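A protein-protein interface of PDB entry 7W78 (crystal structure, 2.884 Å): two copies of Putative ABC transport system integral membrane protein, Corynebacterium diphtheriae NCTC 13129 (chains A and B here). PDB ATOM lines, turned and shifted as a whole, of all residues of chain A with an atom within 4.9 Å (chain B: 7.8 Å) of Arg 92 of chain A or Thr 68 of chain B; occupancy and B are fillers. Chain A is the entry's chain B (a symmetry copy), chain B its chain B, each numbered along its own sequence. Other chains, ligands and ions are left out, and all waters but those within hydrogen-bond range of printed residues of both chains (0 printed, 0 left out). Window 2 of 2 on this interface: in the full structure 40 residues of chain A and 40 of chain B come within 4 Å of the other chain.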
ATOM      1  N   GLN A  90      -9.944  14.973  25.024  1.00  0.00           N
ATOM      2  CA  GLN A  90     -10.037  15.021  23.573  1.00  0.00           C
ATOM      3  C   GLN A  90      -9.260  16.240  23.105  1.00  0.00           C
ATOM      4  O   GLN A  90      -9.509  17.353  23.579  1.00  0.00           O
ATOM      5  CB  GLN A  90     -11.491  15.111  23.097  1.00  0.00           C
ATOM      6  CG  GLN A  90     -12.409  14.009  23.595  1.00  0.00           C
ATOM      7  CD  GLN A  90     -13.879  14.340  23.382  1.00  0.00           C
ATOM      8  OE1 GLN A  90     -14.610  14.618  24.336  1.00  0.00           O
ATOM      9  NE2 GLN A  90     -14.319  14.308  22.125  1.00  0.00           N
ATOM     10  N   THR A  91      -8.318  16.044  22.190  1.00  0.00           N
ATOM     11  CA  THR A  91      -7.546  17.185  21.724  1.00  0.00           C
ATOM     12  C   THR A  91      -7.118  16.987  20.283  1.00  0.00           C
ATOM     13  O   THR A  91      -7.305  15.923  19.686  1.00  0.00           O
ATOM     14  CB  THR A  91      -6.313  17.442  22.595  1.00  0.00           C
ATOM     15  OG1 THR A  91      -5.587  18.554  22.059  1.00  0.00           O
ATOM     16  CG2 THR A  91      -5.409  16.230  22.617  1.00  0.00           C
ATOM     17  N   ARG A  92      -6.529  18.044  19.738  1.00  0.00           N
ATOM     18  CA  ARG A  92      -6.057  18.041  18.367  1.00  0.00           C
ATOM     19  C   ARG A  92      -4.686  17.387  18.293  1.00  0.00           C
ATOM     20  O   ARG A  92      -3.769  17.755  19.034  1.00  0.00           O
ATOM     21  CB  ARG A  92      -5.992  19.468  17.837  1.00  0.00           C
ATOM     22  CG  ARG A  92      -5.733  19.554  16.357  1.00  0.00           C
ATOM     23  CD  ARG A  92      -5.669  20.995  15.917  1.00  0.00           C
ATOM     24  NE  ARG A  92      -6.314  21.179  14.626  1.00  0.00           N
ATOM     25  CZ  ARG A  92      -5.688  21.084  13.460  1.00  0.00           C
ATOM     26  NH1 ARG A  92      -4.390  20.805  13.422  1.00  0.00           N
ATOM     27  NH2 ARG A  92      -6.358  21.266  12.329  1.00  0.00           N
ATOM     28  N   ILE A  93      -4.553  16.408  17.409  1.00  0.00           N
ATOM     29  CA  ILE A  93      -3.271  15.803  17.100  1.00  0.00           C
ATOM     30  C   ILE A  93      -2.876  16.261  15.705  1.00  0.00           C
ATOM     31  O   ILE A  93      -3.708  16.299  14.791  1.00  0.00           O
ATOM     32  CB  ILE A  93      -3.316  14.265  17.210  1.00  0.00           C
ATOM     33  CG1 ILE A  93      -1.925  13.677  16.987  1.00  0.00           C
ATOM     34  CG2 ILE A  93      -4.341  13.676  16.249  1.00  0.00           C
ATOM     35  CD1 ILE A  93      -1.790  12.258  17.478  1.00  0.00           C
ATOM     36  N   GLU A  94      -1.616  16.648  15.554  1.00  0.00           N
ATOM     37  CA  GLU A  94      -1.193  17.310  14.335  1.00  0.00           C
ATOM     38  C   GLU A  94       0.183  16.809  13.943  1.00  0.00           C
ATOM     39  O   GLU A  94       1.124  16.878  14.739  1.00  0.00           O
ATOM     40  CB  GLU A  94      -1.181  18.829  14.520  1.00  0.00           C
ATOM     41  CG  GLU A  94      -0.902  19.605  13.254  1.00  0.00           C
ATOM     42  CD  GLU A  94      -1.139  21.093  13.443  1.00  0.00           C
ATOM     43  OE1 GLU A  94      -1.727  21.470  14.481  1.00  0.00           O
ATOM     44  OE2 GLU A  94      -0.739  21.881  12.561  1.00  0.00           O
ATOM     45  N   ASN A  98      -0.778  16.018   8.182  1.00  0.00           N
ATOM     46  CA  ASN A  98      -2.212  15.868   8.416  1.00  0.00           C
ATOM     47  C   ASN A  98      -2.503  16.168   9.885  1.00  0.00           C
ATOM     48  O   ASN A  98      -1.597  16.450  10.673  1.00  0.00           O
ATOM     49  CB  ASN A  98      -2.679  14.468   8.013  1.00  0.00           C
ATOM     50  CG  ASN A  98      -4.118  14.449   7.553  1.00  0.00           C
ATOM     51  OD1 ASN A  98      -5.018  14.909   8.260  1.00  0.00           O
ATOM     52  ND2 ASN A  98      -4.339  13.964   6.335  1.00  0.00           N
ATOM     53  N   ALA A  99      -3.786  16.106  10.245  1.00  0.00           N
ATOM     54  CA  ALA A  99      -4.213  16.403  11.604  1.00  0.00           C
ATOM     55  C   ALA A  99      -5.536  15.709  11.882  1.00  0.00           C
ATOM     56  O   ALA A  99      -6.166  15.141  10.986  1.00  0.00           O
ATOM     57  CB  ALA A  99      -4.343  17.911  11.835  1.00  0.00           C
ATOM     58  N   ASN A 100      -5.958  15.782  13.141  1.00  0.00           N
ATOM     59  CA  ASN A 100      -7.224  15.225  13.595  1.00  0.00           C
ATOM     60  C   ASN A 100      -7.439  15.653  15.039  1.00  0.00           C
ATOM     61  O   ASN A 100      -6.535  16.179  15.693  1.00  0.00           O
ATOM     62  CB  ASN A 100      -7.247  13.697  13.478  1.00  0.00           C
ATOM     63  CG  ASN A 100      -8.649  13.146  13.310  1.00  0.00           C
ATOM     64  OD1 ASN A 100      -9.628  13.798  13.675  1.00  0.00           O
ATOM     65  ND2 ASN A 100      -8.753  11.942  12.751  1.00  0.00           N
ATOM     66  N   THR A 101      -8.659  15.438  15.521  1.00  0.00           N
ATOM     67  CA  THR A 101      -8.953  15.437  16.945  1.00  0.00           C
ATOM     68  C   THR A 101      -9.076  13.988  17.398  1.00  0.00           C
ATOM     69  O   THR A 101      -9.647  13.154  16.688  1.00  0.00           O
ATOM     70  CB  THR A 101     -10.237  16.217  17.255  1.00  0.00           C
ATOM     71  OG1 THR A 101      -9.958  17.620  17.232  1.00  0.00           O
ATOM     72  CG2 THR A 101     -10.791  15.849  18.629  1.00  0.00           C
ATOM     73  N   PHE A 134      -2.745   7.317   9.316  1.00  0.00           N
ATOM     74  CA  PHE A 134      -3.464   8.525   8.923  1.00  0.00           C
ATOM     75  C   PHE A 134      -2.559   9.750   8.965  1.00  0.00           C
ATOM     76  O   PHE A 134      -2.531  10.553   8.026  1.00  0.00           O
ATOM     77  CB  PHE A 134      -4.679   8.716   9.831  1.00  0.00           C
ATOM     78  CG  PHE A 134      -5.397  10.011   9.614  1.00  0.00           C
ATOM     79  CD1 PHE A 134      -6.028  10.273   8.411  1.00  0.00           C
ATOM     80  CD2 PHE A 134      -5.447  10.965  10.616  1.00  0.00           C
ATOM     81  CE1 PHE A 134      -6.689  11.464   8.207  1.00  0.00           C
ATOM     82  CE2 PHE A 134      -6.110  12.156  10.418  1.00  0.00           C
ATOM     83  CZ  PHE A 134      -6.732  12.408   9.211  1.00  0.00           C
ATOM     84  N   THR A 144       2.388  17.355  17.161  1.00  0.00           N
ATOM     85  CA  THR A 144       1.797  18.311  18.082  1.00  0.00           C
ATOM     86  C   THR A 144       0.534  17.689  18.663  1.00  0.00           C
ATOM     87  O   THR A 144      -0.380  17.311  17.921  1.00  0.00           O
ATOM     88  CB  THR A 144       1.484  19.643  17.403  1.00  0.00           C
ATOM     89  OG1 THR A 144       2.578  20.023  16.559  1.00  0.00           O
ATOM     90  CG2 THR A 144       1.294  20.723  18.454  1.00  0.00           C
ATOM     91  N   LEU A 145       0.500  17.557  19.985  1.00  0.00           N
ATOM     92  CA  LEU A 145      -0.644  17.014  20.707  1.00  0.00           C
ATOM     93  C   LEU A 145      -1.107  18.080  21.689  1.00  0.00           C
ATOM     94  O   LEU A 145      -0.386  18.406  22.638  1.00  0.00           O
ATOM     95  CB  LEU A 145      -0.270  15.720  21.427  1.00  0.00           C
ATOM     96  CG  LEU A 145      -1.399  14.825  21.931  1.00  0.00           C
ATOM     97  CD1 LEU A 145      -2.253  14.348  20.768  1.00  0.00           C
ATOM     98  CD2 LEU A 145      -0.830  13.644  22.706  1.00  0.00           C
ATOM     99  N   GLY A 146      -2.292  18.632  21.454  1.00  0.00           N
ATOM    100  CA  GLY A 146      -2.777  19.706  22.303  1.00  0.00           C
ATOM    101  C   GLY A 146      -1.877  20.921  22.316  1.00  0.00           C
ATOM    102  O   GLY A 146      -1.706  21.555  23.364  1.00  0.00           O
ATOM    103  N   GLY A 147      -1.285  21.256  21.172  1.00  0.00           N
ATOM    104  CA  GLY A 147      -0.376  22.376  21.087  1.00  0.00           C
ATOM    105  C   GLY A 147       1.022  22.117  21.609  1.00  0.00           C
ATOM    106  O   GLY A 147       1.854  23.032  21.573  1.00  0.00           O
ATOM    107  N   PHE B  57     -12.232  21.950  -1.754  1.00  0.00           N
ATOM    108  CA  PHE B  57     -11.303  21.566  -0.707  1.00  0.00           C
ATOM    109  C   PHE B  57      -9.907  22.065  -1.056  1.00  0.00           C
ATOM    110  O   PHE B  57      -9.694  22.755  -2.057  1.00  0.00           O
ATOM    111  CB  PHE B  57     -11.317  20.050  -0.510  1.00  0.00           C
ATOM    112  CG  PHE B  57     -12.475  19.563   0.305  1.00  0.00           C
ATOM    113  CD1 PHE B  57     -13.720  19.378  -0.274  1.00  0.00           C
ATOM    114  CD2 PHE B  57     -12.319  19.291   1.653  1.00  0.00           C
ATOM    115  CE1 PHE B  57     -14.788  18.933   0.478  1.00  0.00           C
ATOM    116  CE2 PHE B  57     -13.384  18.844   2.409  1.00  0.00           C
ATOM    117  CZ  PHE B  57     -14.620  18.664   1.820  1.00  0.00           C
ATOM    118  N   THR B  58      -8.950  21.713  -0.204  1.00  0.00           N
ATOM    119  CA  THR B  58      -7.546  21.974  -0.478  1.00  0.00           C
ATOM    120  C   THR B  58      -6.743  20.755  -0.059  1.00  0.00           C
ATOM    121  O   THR B  58      -6.939  20.220   1.037  1.00  0.00           O
ATOM    122  CB  THR B  58      -7.052  23.232   0.248  1.00  0.00           C
ATOM    123  OG1 THR B  58      -7.571  24.393  -0.413  1.00  0.00           O
ATOM    124  CG2 THR B  58      -5.530  23.296   0.238  1.00  0.00           C
ATOM    125  N   PRO B  65      -9.310  14.761  -0.301  1.00  0.00           N
ATOM    126  CA  PRO B  65      -9.639  15.907   0.554  1.00  0.00           C
ATOM    127  C   PRO B  65     -10.037  15.449   1.947  1.00  0.00           C
ATOM    128  O   PRO B  65     -10.657  14.398   2.126  1.00  0.00           O
ATOM    129  CB  PRO B  65     -10.805  16.577  -0.181  1.00  0.00           C
ATOM    130  CG  PRO B  65     -11.365  15.509  -1.071  1.00  0.00           C
ATOM    131  CD  PRO B  65     -10.191  14.676  -1.476  1.00  0.00           C
ATOM    132  N   GLU B  66      -9.648  16.241   2.944  1.00  0.00           N
ATOM    133  CA  GLU B  66      -9.959  15.955   4.336  1.00  0.00           C
ATOM    134  C   GLU B  66     -10.391  17.245   5.008  1.00  0.00           C
ATOM    135  O   GLU B  66      -9.746  18.281   4.826  1.00  0.00           O
ATOM    136  CB  GLU B  66      -8.751  15.365   5.072  1.00  0.00           C
ATOM    137  CG  GLU B  66      -8.120  14.163   4.395  1.00  0.00           C
ATOM    138  CD  GLU B  66      -8.437  12.865   5.112  1.00  0.00           C
ATOM    139  OE1 GLU B  66      -7.666  11.896   4.952  1.00  0.00           O
ATOM    140  OE2 GLU B  66      -9.458  12.812   5.833  1.00  0.00           O
ATOM    141  N   PHE B  67     -11.476  17.185   5.780  1.00  0.00           N
ATOM    142  CA  PHE B  67     -11.900  18.371   6.511  1.00  0.00           C
ATOM    143  C   PHE B  67     -10.868  18.786   7.550  1.00  0.00           C
ATOM    144  O   PHE B  67     -10.783  19.966   7.905  1.00  0.00           O
ATOM    145  CB  PHE B  67     -13.261  18.132   7.164  1.00  0.00           C
ATOM    146  CG  PHE B  67     -14.404  18.672   6.365  1.00  0.00           C
ATOM    147  CD1 PHE B  67     -14.648  20.033   6.334  1.00  0.00           C
ATOM    148  CD2 PHE B  67     -15.225  17.827   5.633  1.00  0.00           C
ATOM    149  CE1 PHE B  67     -15.693  20.546   5.595  1.00  0.00           C
ATOM    150  CE2 PHE B  67     -16.272  18.333   4.890  1.00  0.00           C
ATOM    151  CZ  PHE B  67     -16.507  19.696   4.871  1.00  0.00           C
ATOM    152  N   THR B  68     -10.058  17.842   8.028  1.00  0.00           N
ATOM    153  CA  THR B  68      -9.062  18.143   9.045  1.00  0.00           C
ATOM    154  C   THR B  68      -7.811  18.817   8.491  1.00  0.00           C
ATOM    155  O   THR B  68      -6.992  19.296   9.282  1.00  0.00           O
ATOM    156  CB  THR B  68      -8.651  16.864   9.781  1.00  0.00           C
ATOM    157  OG1 THR B  68      -8.309  15.847   8.830  1.00  0.00           O
ATOM    158  CG2 THR B  68      -9.787  16.370  10.663  1.00  0.00           C
ATOM    159  N   SER B  69      -7.640  18.873   7.168  1.00  0.00           N
ATOM    160  CA  SER B  69      -6.389  19.349   6.589  1.00  0.00           C
ATOM    161  C   SER B  69      -6.590  20.366   5.472  1.00  0.00           C
ATOM    162  O   SER B  69      -5.613  20.737   4.812  1.00  0.00           O
ATOM    163  CB  SER B  69      -5.563  18.168   6.069  1.00  0.00           C
ATOM    164  OG  SER B  69      -5.486  17.141   7.041  1.00  0.00           O
ATOM    165  N   SER B  70      -7.815  20.822   5.239  1.00  0.00           N
ATOM    166  CA  SER B  70      -8.094  21.820   4.218  1.00  0.00           C
ATOM    167  C   SER B  70      -8.167  23.202   4.854  1.00  0.00           C
ATOM    168  O   SER B  70      -8.691  23.360   5.960  1.00  0.00           O
ATOM    169  CB  SER B  70      -9.405  21.503   3.495  1.00  0.00           C
ATOM    170  OG  SER B  70      -9.725  22.511   2.551  1.00  0.00           O
ATOM    171  N   GLU B  71      -7.615  24.198   4.164  1.00  0.00           N
ATOM    172  CA  GLU B  71      -7.786  25.589   4.560  1.00  0.00           C
ATOM    173  C   GLU B  71      -7.959  26.462   3.330  1.00  0.00           C
ATOM    174  O   GLU B  71      -7.297  26.252   2.309  1.00  0.00           O
ATOM    175  CB  GLU B  71      -6.609  26.145   5.368  1.00  0.00           C
ATOM    176  CG  GLU B  71      -5.842  25.186   6.226  1.00  0.00           C
ATOM    177  CD  GLU B  71      -5.073  25.917   7.287  1.00  0.00           C
ATOM    178  OE1 GLU B  71      -3.930  26.338   7.009  1.00  0.00           O
ATOM    179  OE2 GLU B  71      -5.618  26.084   8.396  1.00  0.00           O
ATOM    180  N   VAL B  88     -14.529  24.728   9.658  1.00  0.00           N
ATOM    181  CA  VAL B  88     -14.929  23.569  10.448  1.00  0.00           C
ATOM    182  C   VAL B  88     -13.798  23.235  11.407  1.00  0.00           C
ATOM    183  O   VAL B  88     -12.671  22.960  10.976  1.00  0.00           O
ATOM    184  CB  VAL B  88     -15.268  22.354   9.570  1.00  0.00           C
ATOM    185  CG1 VAL B  88     -15.792  21.221  10.437  1.00  0.00           C
ATOM    186  CG2 VAL B  88     -16.289  22.724   8.505  1.00  0.00           C
ATOM    187  N   SER B  89     -14.101  23.254  12.702  1.00  0.00           N
ATOM    188  CA  SER B  89     -13.147  22.874  13.730  1.00  0.00           C
ATOM    189  C   SER B  89     -13.872  22.088  14.812  1.00  0.00           C
ATOM    190  O   SER B  89     -15.083  22.221  15.003  1.00  0.00           O
ATOM    191  CB  SER B  89     -12.455  24.099  14.347  1.00  0.00           C
ATOM    192  OG  SER B  89     -11.914  24.947  13.349  1.00  0.00           O
ATOM    193  N   GLN B  90     -13.112  21.244  15.501  1.00  0.00           N
ATOM    194  CA  GLN B  90     -13.533  20.636  16.755  1.00  0.00           C
ATOM    195  C   GLN B  90     -12.662  21.214  17.858  1.00  0.00           C
ATOM    196  O   GLN B  90     -11.431  21.172  17.762  1.00  0.00           O
ATOM    197  CB  GLN B  90     -13.395  19.110  16.724  1.00  0.00           C
ATOM    198  CG  GLN B  90     -14.127  18.413  15.589  1.00  0.00           C
ATOM    199  CD  GLN B  90     -13.675  16.971  15.410  1.00  0.00           C
ATOM    200  OE1 GLN B  90     -12.996  16.637  14.435  1.00  0.00           O
ATOM    201  NE2 GLN B  90     -14.056  16.108  16.350  1.00  0.00           N
ATOM    202  N   THR B  91     -13.282  21.760  18.897  1.00  0.00           N
ATOM    203  CA  THR B  91     -12.483  22.333  19.968  1.00  0.00           C
ATOM    204  C   THR B  91     -13.205  22.210  21.296  1.00  0.00           C
ATOM    205  O   THR B  91     -14.368  21.803  21.373  1.00  0.00           O
ATOM    206  CB  THR B  91     -12.134  23.801  19.707  1.00  0.00           C
ATOM    207  OG1 THR B  91     -11.379  24.305  20.814  1.00  0.00           O
ATOM    208  CG2 THR B  91     -13.389  24.630  19.550  1.00  0.00           C
ATOM    209  N   THR B 101     -15.997  19.033  24.388  1.00  0.00           N
ATOM    210  CA  THR B 101     -15.486  19.271  23.047  1.00  0.00           C
ATOM    211  C   THR B 101     -16.672  19.293  22.090  1.00  0.00           C
ATOM    212  O   THR B 101     -17.601  18.491  22.222  1.00  0.00           O
ATOM    213  CB  THR B 101     -14.471  18.198  22.634  1.00  0.00           C
ATOM    214  OG1 THR B 101     -13.210  18.475  23.251  1.00  0.00           O
ATOM    215  CG2 THR B 101     -14.282  18.169  21.120  1.00  0.00           C
ATOM    216  N   TYR B 161     -22.003  17.705  13.327  1.00  0.00           N
ATOM    217  CA  TYR B 161     -20.762  17.369  12.649  1.00  0.00           C
ATOM    218  C   TYR B 161     -19.957  16.496  13.597  1.00  0.00           C
ATOM    219  O   TYR B 161     -19.762  16.870  14.757  1.00  0.00           O
ATOM    220  CB  TYR B 161     -19.972  18.628  12.266  1.00  0.00           C
ATOM    221  CG  TYR B 161     -18.623  18.350  11.647  1.00  0.00           C
ATOM    222  CD1 TYR B 161     -17.494  18.186  12.438  1.00  0.00           C
ATOM    223  CD2 TYR B 161     -18.482  18.251  10.272  1.00  0.00           C
ATOM    224  CE1 TYR B 161     -16.263  17.926  11.878  1.00  0.00           C
ATOM    225  CE2 TYR B 161     -17.254  17.993   9.700  1.00  0.00           C
ATOM    226  CZ  TYR B 161     -16.149  17.831  10.508  1.00  0.00           C
ATOM    227  OH  TYR B 161     -14.922  17.574   9.945  1.00  0.00           O
ATOM    228  N   SER B 178      -9.751  28.666  16.336  1.00  0.00           N
ATOM    229  CA  SER B 178      -9.007  27.600  15.674  1.00  0.00           C
ATOM    230  C   SER B 178      -7.564  27.984  15.353  1.00  0.00           C
ATOM    231  O   SER B 178      -6.849  27.189  14.732  1.00  0.00           O
ATOM    232  CB  SER B 178      -9.724  27.147  14.395  1.00  0.00           C
ATOM    233  OG  SER B 178     -10.790  28.010  14.053  1.00  0.00           O
ATOM    234  N   HIS B 179      -7.126  29.180  15.753  1.00  0.00           N
ATOM    235  CA  HIS B 179      -5.719  29.586  15.691  1.00  0.00           C
ATOM    236  C   HIS B 179      -5.178  29.549  14.258  1.00  0.00           C
ATOM    237  O   HIS B 179      -4.184  28.882  13.965  1.00  0.00           O
ATOM    238  CB  HIS B 179      -4.863  28.704  16.612  1.00  0.00           C
ATOM    239  CG  HIS B 179      -5.418  28.536  17.996  1.00  0.00           C
ATOM    240  ND1 HIS B 179      -5.217  29.459  19.001  1.00  0.00           N
ATOM    241  CD2 HIS B 179      -6.158  27.542  18.542  1.00  0.00           C
ATOM    242  CE1 HIS B 179      -5.811  29.042  20.105  1.00  0.00           C
ATOM    243  NE2 HIS B 179      -6.390  27.882  19.853  1.00  0.00           N
ATOM    244  N   THR B 185     -12.367  26.475   6.049  1.00  0.00           N
ATOM    245  CA  THR B 185     -11.870  25.139   5.754  1.00  0.00           C
ATOM    246  C   THR B 185     -12.241  24.678   4.350  1.00  0.00           C
ATOM    247  O   THR B 185     -11.453  23.984   3.703  1.00  0.00           O
ATOM    248  CB  THR B 185     -12.399  24.139   6.793  1.00  0.00           C
ATOM    249  OG1 THR B 185     -12.018  24.565   8.109  1.00  0.00           O
ATOM    250  CG2 THR B 185     -11.845  22.744   6.546  1.00  0.00           C
ATOM    251  N   ALA B 212     -14.633  13.224   3.106  1.00  0.00           N
ATOM    252  CA  ALA B 212     -13.623  14.071   3.721  1.00  0.00           C
ATOM    253  C   ALA B 212     -13.787  14.215   5.232  1.00  0.00           C
ATOM    254  O   ALA B 212     -12.935  14.842   5.871  1.00  0.00           O
ATOM    255  CB  ALA B 212     -13.635  15.456   3.071  1.00  0.00           C
ATOM    256  N   MET B 213     -14.854  13.663   5.820  1.00  0.00           N
ATOM    257  CA  MET B 213     -15.029  13.701   7.268  1.00  0.00           C
ATOM    258  C   MET B 213     -14.510  12.407   7.872  1.00  0.00           C
ATOM    259  O   MET B 213     -15.019  11.330   7.524  1.00  0.00           O
ATOM    260  CB  MET B 213     -16.496  13.901   7.640  1.00  0.00           C
ATOM    261  CG  MET B 213     -17.284  14.797   6.700  1.00  0.00           C
ATOM    262  SD  MET B 213     -19.038  14.804   7.128  1.00  0.00           S
ATOM    263  CE  MET B 213     -19.528  16.424   6.566  1.00  0.00           C
ATOM    264  N   PRO B 214     -13.515  12.453   8.764  1.00  0.00           N
ATOM    265  CA  PRO B 214     -12.947  11.195   9.284  1.00  0.00           C
ATOM    266  C   PRO B 214     -13.938  10.356  10.074  1.00  0.00           C
ATOM    267  O   PRO B 214     -13.975   9.131   9.906  1.00  0.00           O
ATOM    268  CB  PRO B 214     -11.785  11.678  10.163  1.00  0.00           C
ATOM    269  CG  PRO B 214     -11.456  13.049   9.646  1.00  0.00           C
ATOM    270  CD  PRO B 214     -12.776  13.633   9.239  1.00  0.00           C
ATOM    271  N   ALA B 215     -14.750  10.984  10.931  1.00  0.00           N
ATOM    272  CA  ALA B 215     -15.725  10.245  11.730  1.00  0.00           C
ATOM    273  C   ALA B 215     -16.738   9.511  10.866  1.00  0.00           C
ATOM    274  O   ALA B 215     -17.386   8.570  11.340  1.00  0.00           O
ATOM    275  CB  ALA B 215     -16.454  11.199  12.677  1.00  0.00           C
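The side-chain hydroxyl of Thr 68 of chain B is in hydrogen-bond range of the side-chain amide oxygen of Asn 98 of chain A (3.5 Å). The side-chain hydroxyl (OG1) of Thr 68 of chain B lies within hydrogen-bond range of the backbone carbonyl oxygen (O) of Ala 99 of chain A. OD1 of Asn 98 of chain A lies within hydrogen-bond range of OG of Ser 69 of chain B (2.6 Å).
The guanidinium group (NH1) of Arg 92 of chain A is in salt-bridge range of the side-chain carboxylate (OE1) of Glu 94 of chain A (2.9 Å). The backbone carbonyl oxygen (O) of Arg 92 of chain A is in hydrogen-bond range of the backbone NH (N) of Gly 146 of chain A (3.0 Å). N of Ile 93 of chain A lies within hydrogen-bond range of O of Asn 100 of chain A.
Gln 90 of chain A touches Thr 101 of chain B. NH2 of Arg 92 of chain A touches O of Thr 68 of chain B, 3.7 Å away. Ala 99 of chain A touches Ser 69 of chain B (N to OG, 3.8 Å). Asn 100 of chain A touches Thr 68 of chain B. ND2 of Asn 100 of chain A touches CB of Pro 214 of chain B, 3.995 Å away. Thr 101 of chain A touches Gln 90 of chain B (OG1 to CB, 3.8 Å). Glu 66 of chain B touches Phe 134 of chain A (OE1 to CE1, 3.4 Å). CZ of Phe 134 of chain A touches OG1 of Thr 68 of chain B (3.8 Å).
Arg 92 of chain A touches just one residue of chain B: Thr 68 (3.7 Å). Of chain A, only Arg 92 (3.7 Å), Asn 98 (3.5 Å), Ala 99 (3.1 Å), Asn 100 (3.96 Å) and Phe 134 (3.8 Å) come within 4 Å of Thr 68 of chain B. No residue of chain B comes within 4 Å of Thr 91 of chain A. Printed residues of chain A within 4 Å of Gln 90 of chain B: Thr 101. Of the printed residues of chain B, Asn 100 of chain A touches Thr 68 (3.96 Å) and Pro 214 (3.995 Å). Printed residues of chain A within 4 Å of Thr 101 of chain B: Gln 90. Of the printed residues of chain A, Ser 69 of chain B touches Asn 98 and Ala 99. Of the printed residues of chain A, Glu 66 of chain B touches Phe 134. Ile 93 of chain A touches none of the printed residues of chain B. The nearest printed residue of chain A that does not touch Thr 68 of chain B is Thr 101 of chain A (5.1 Å).
Hydrophobic or aromatic side chains of chain B within 4 Å of the printed part of chain A: Pro 214. Hydrophobic or aromatic side chains of chain A that line the printed part of chain B: Ala 99 and Phe 134. Among the printed residues, 11 pairs touch across the chains. Among the printed residues, no Asp or Glu carboxylate lies within 4 Å of a Lys or Arg side-chain nitrogen of the other chain.
Gln 90 of chain A touches Thr 101 of chain B, and with the chains exchanged Thr 101 of chain A touches Gln 90 of chain B.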
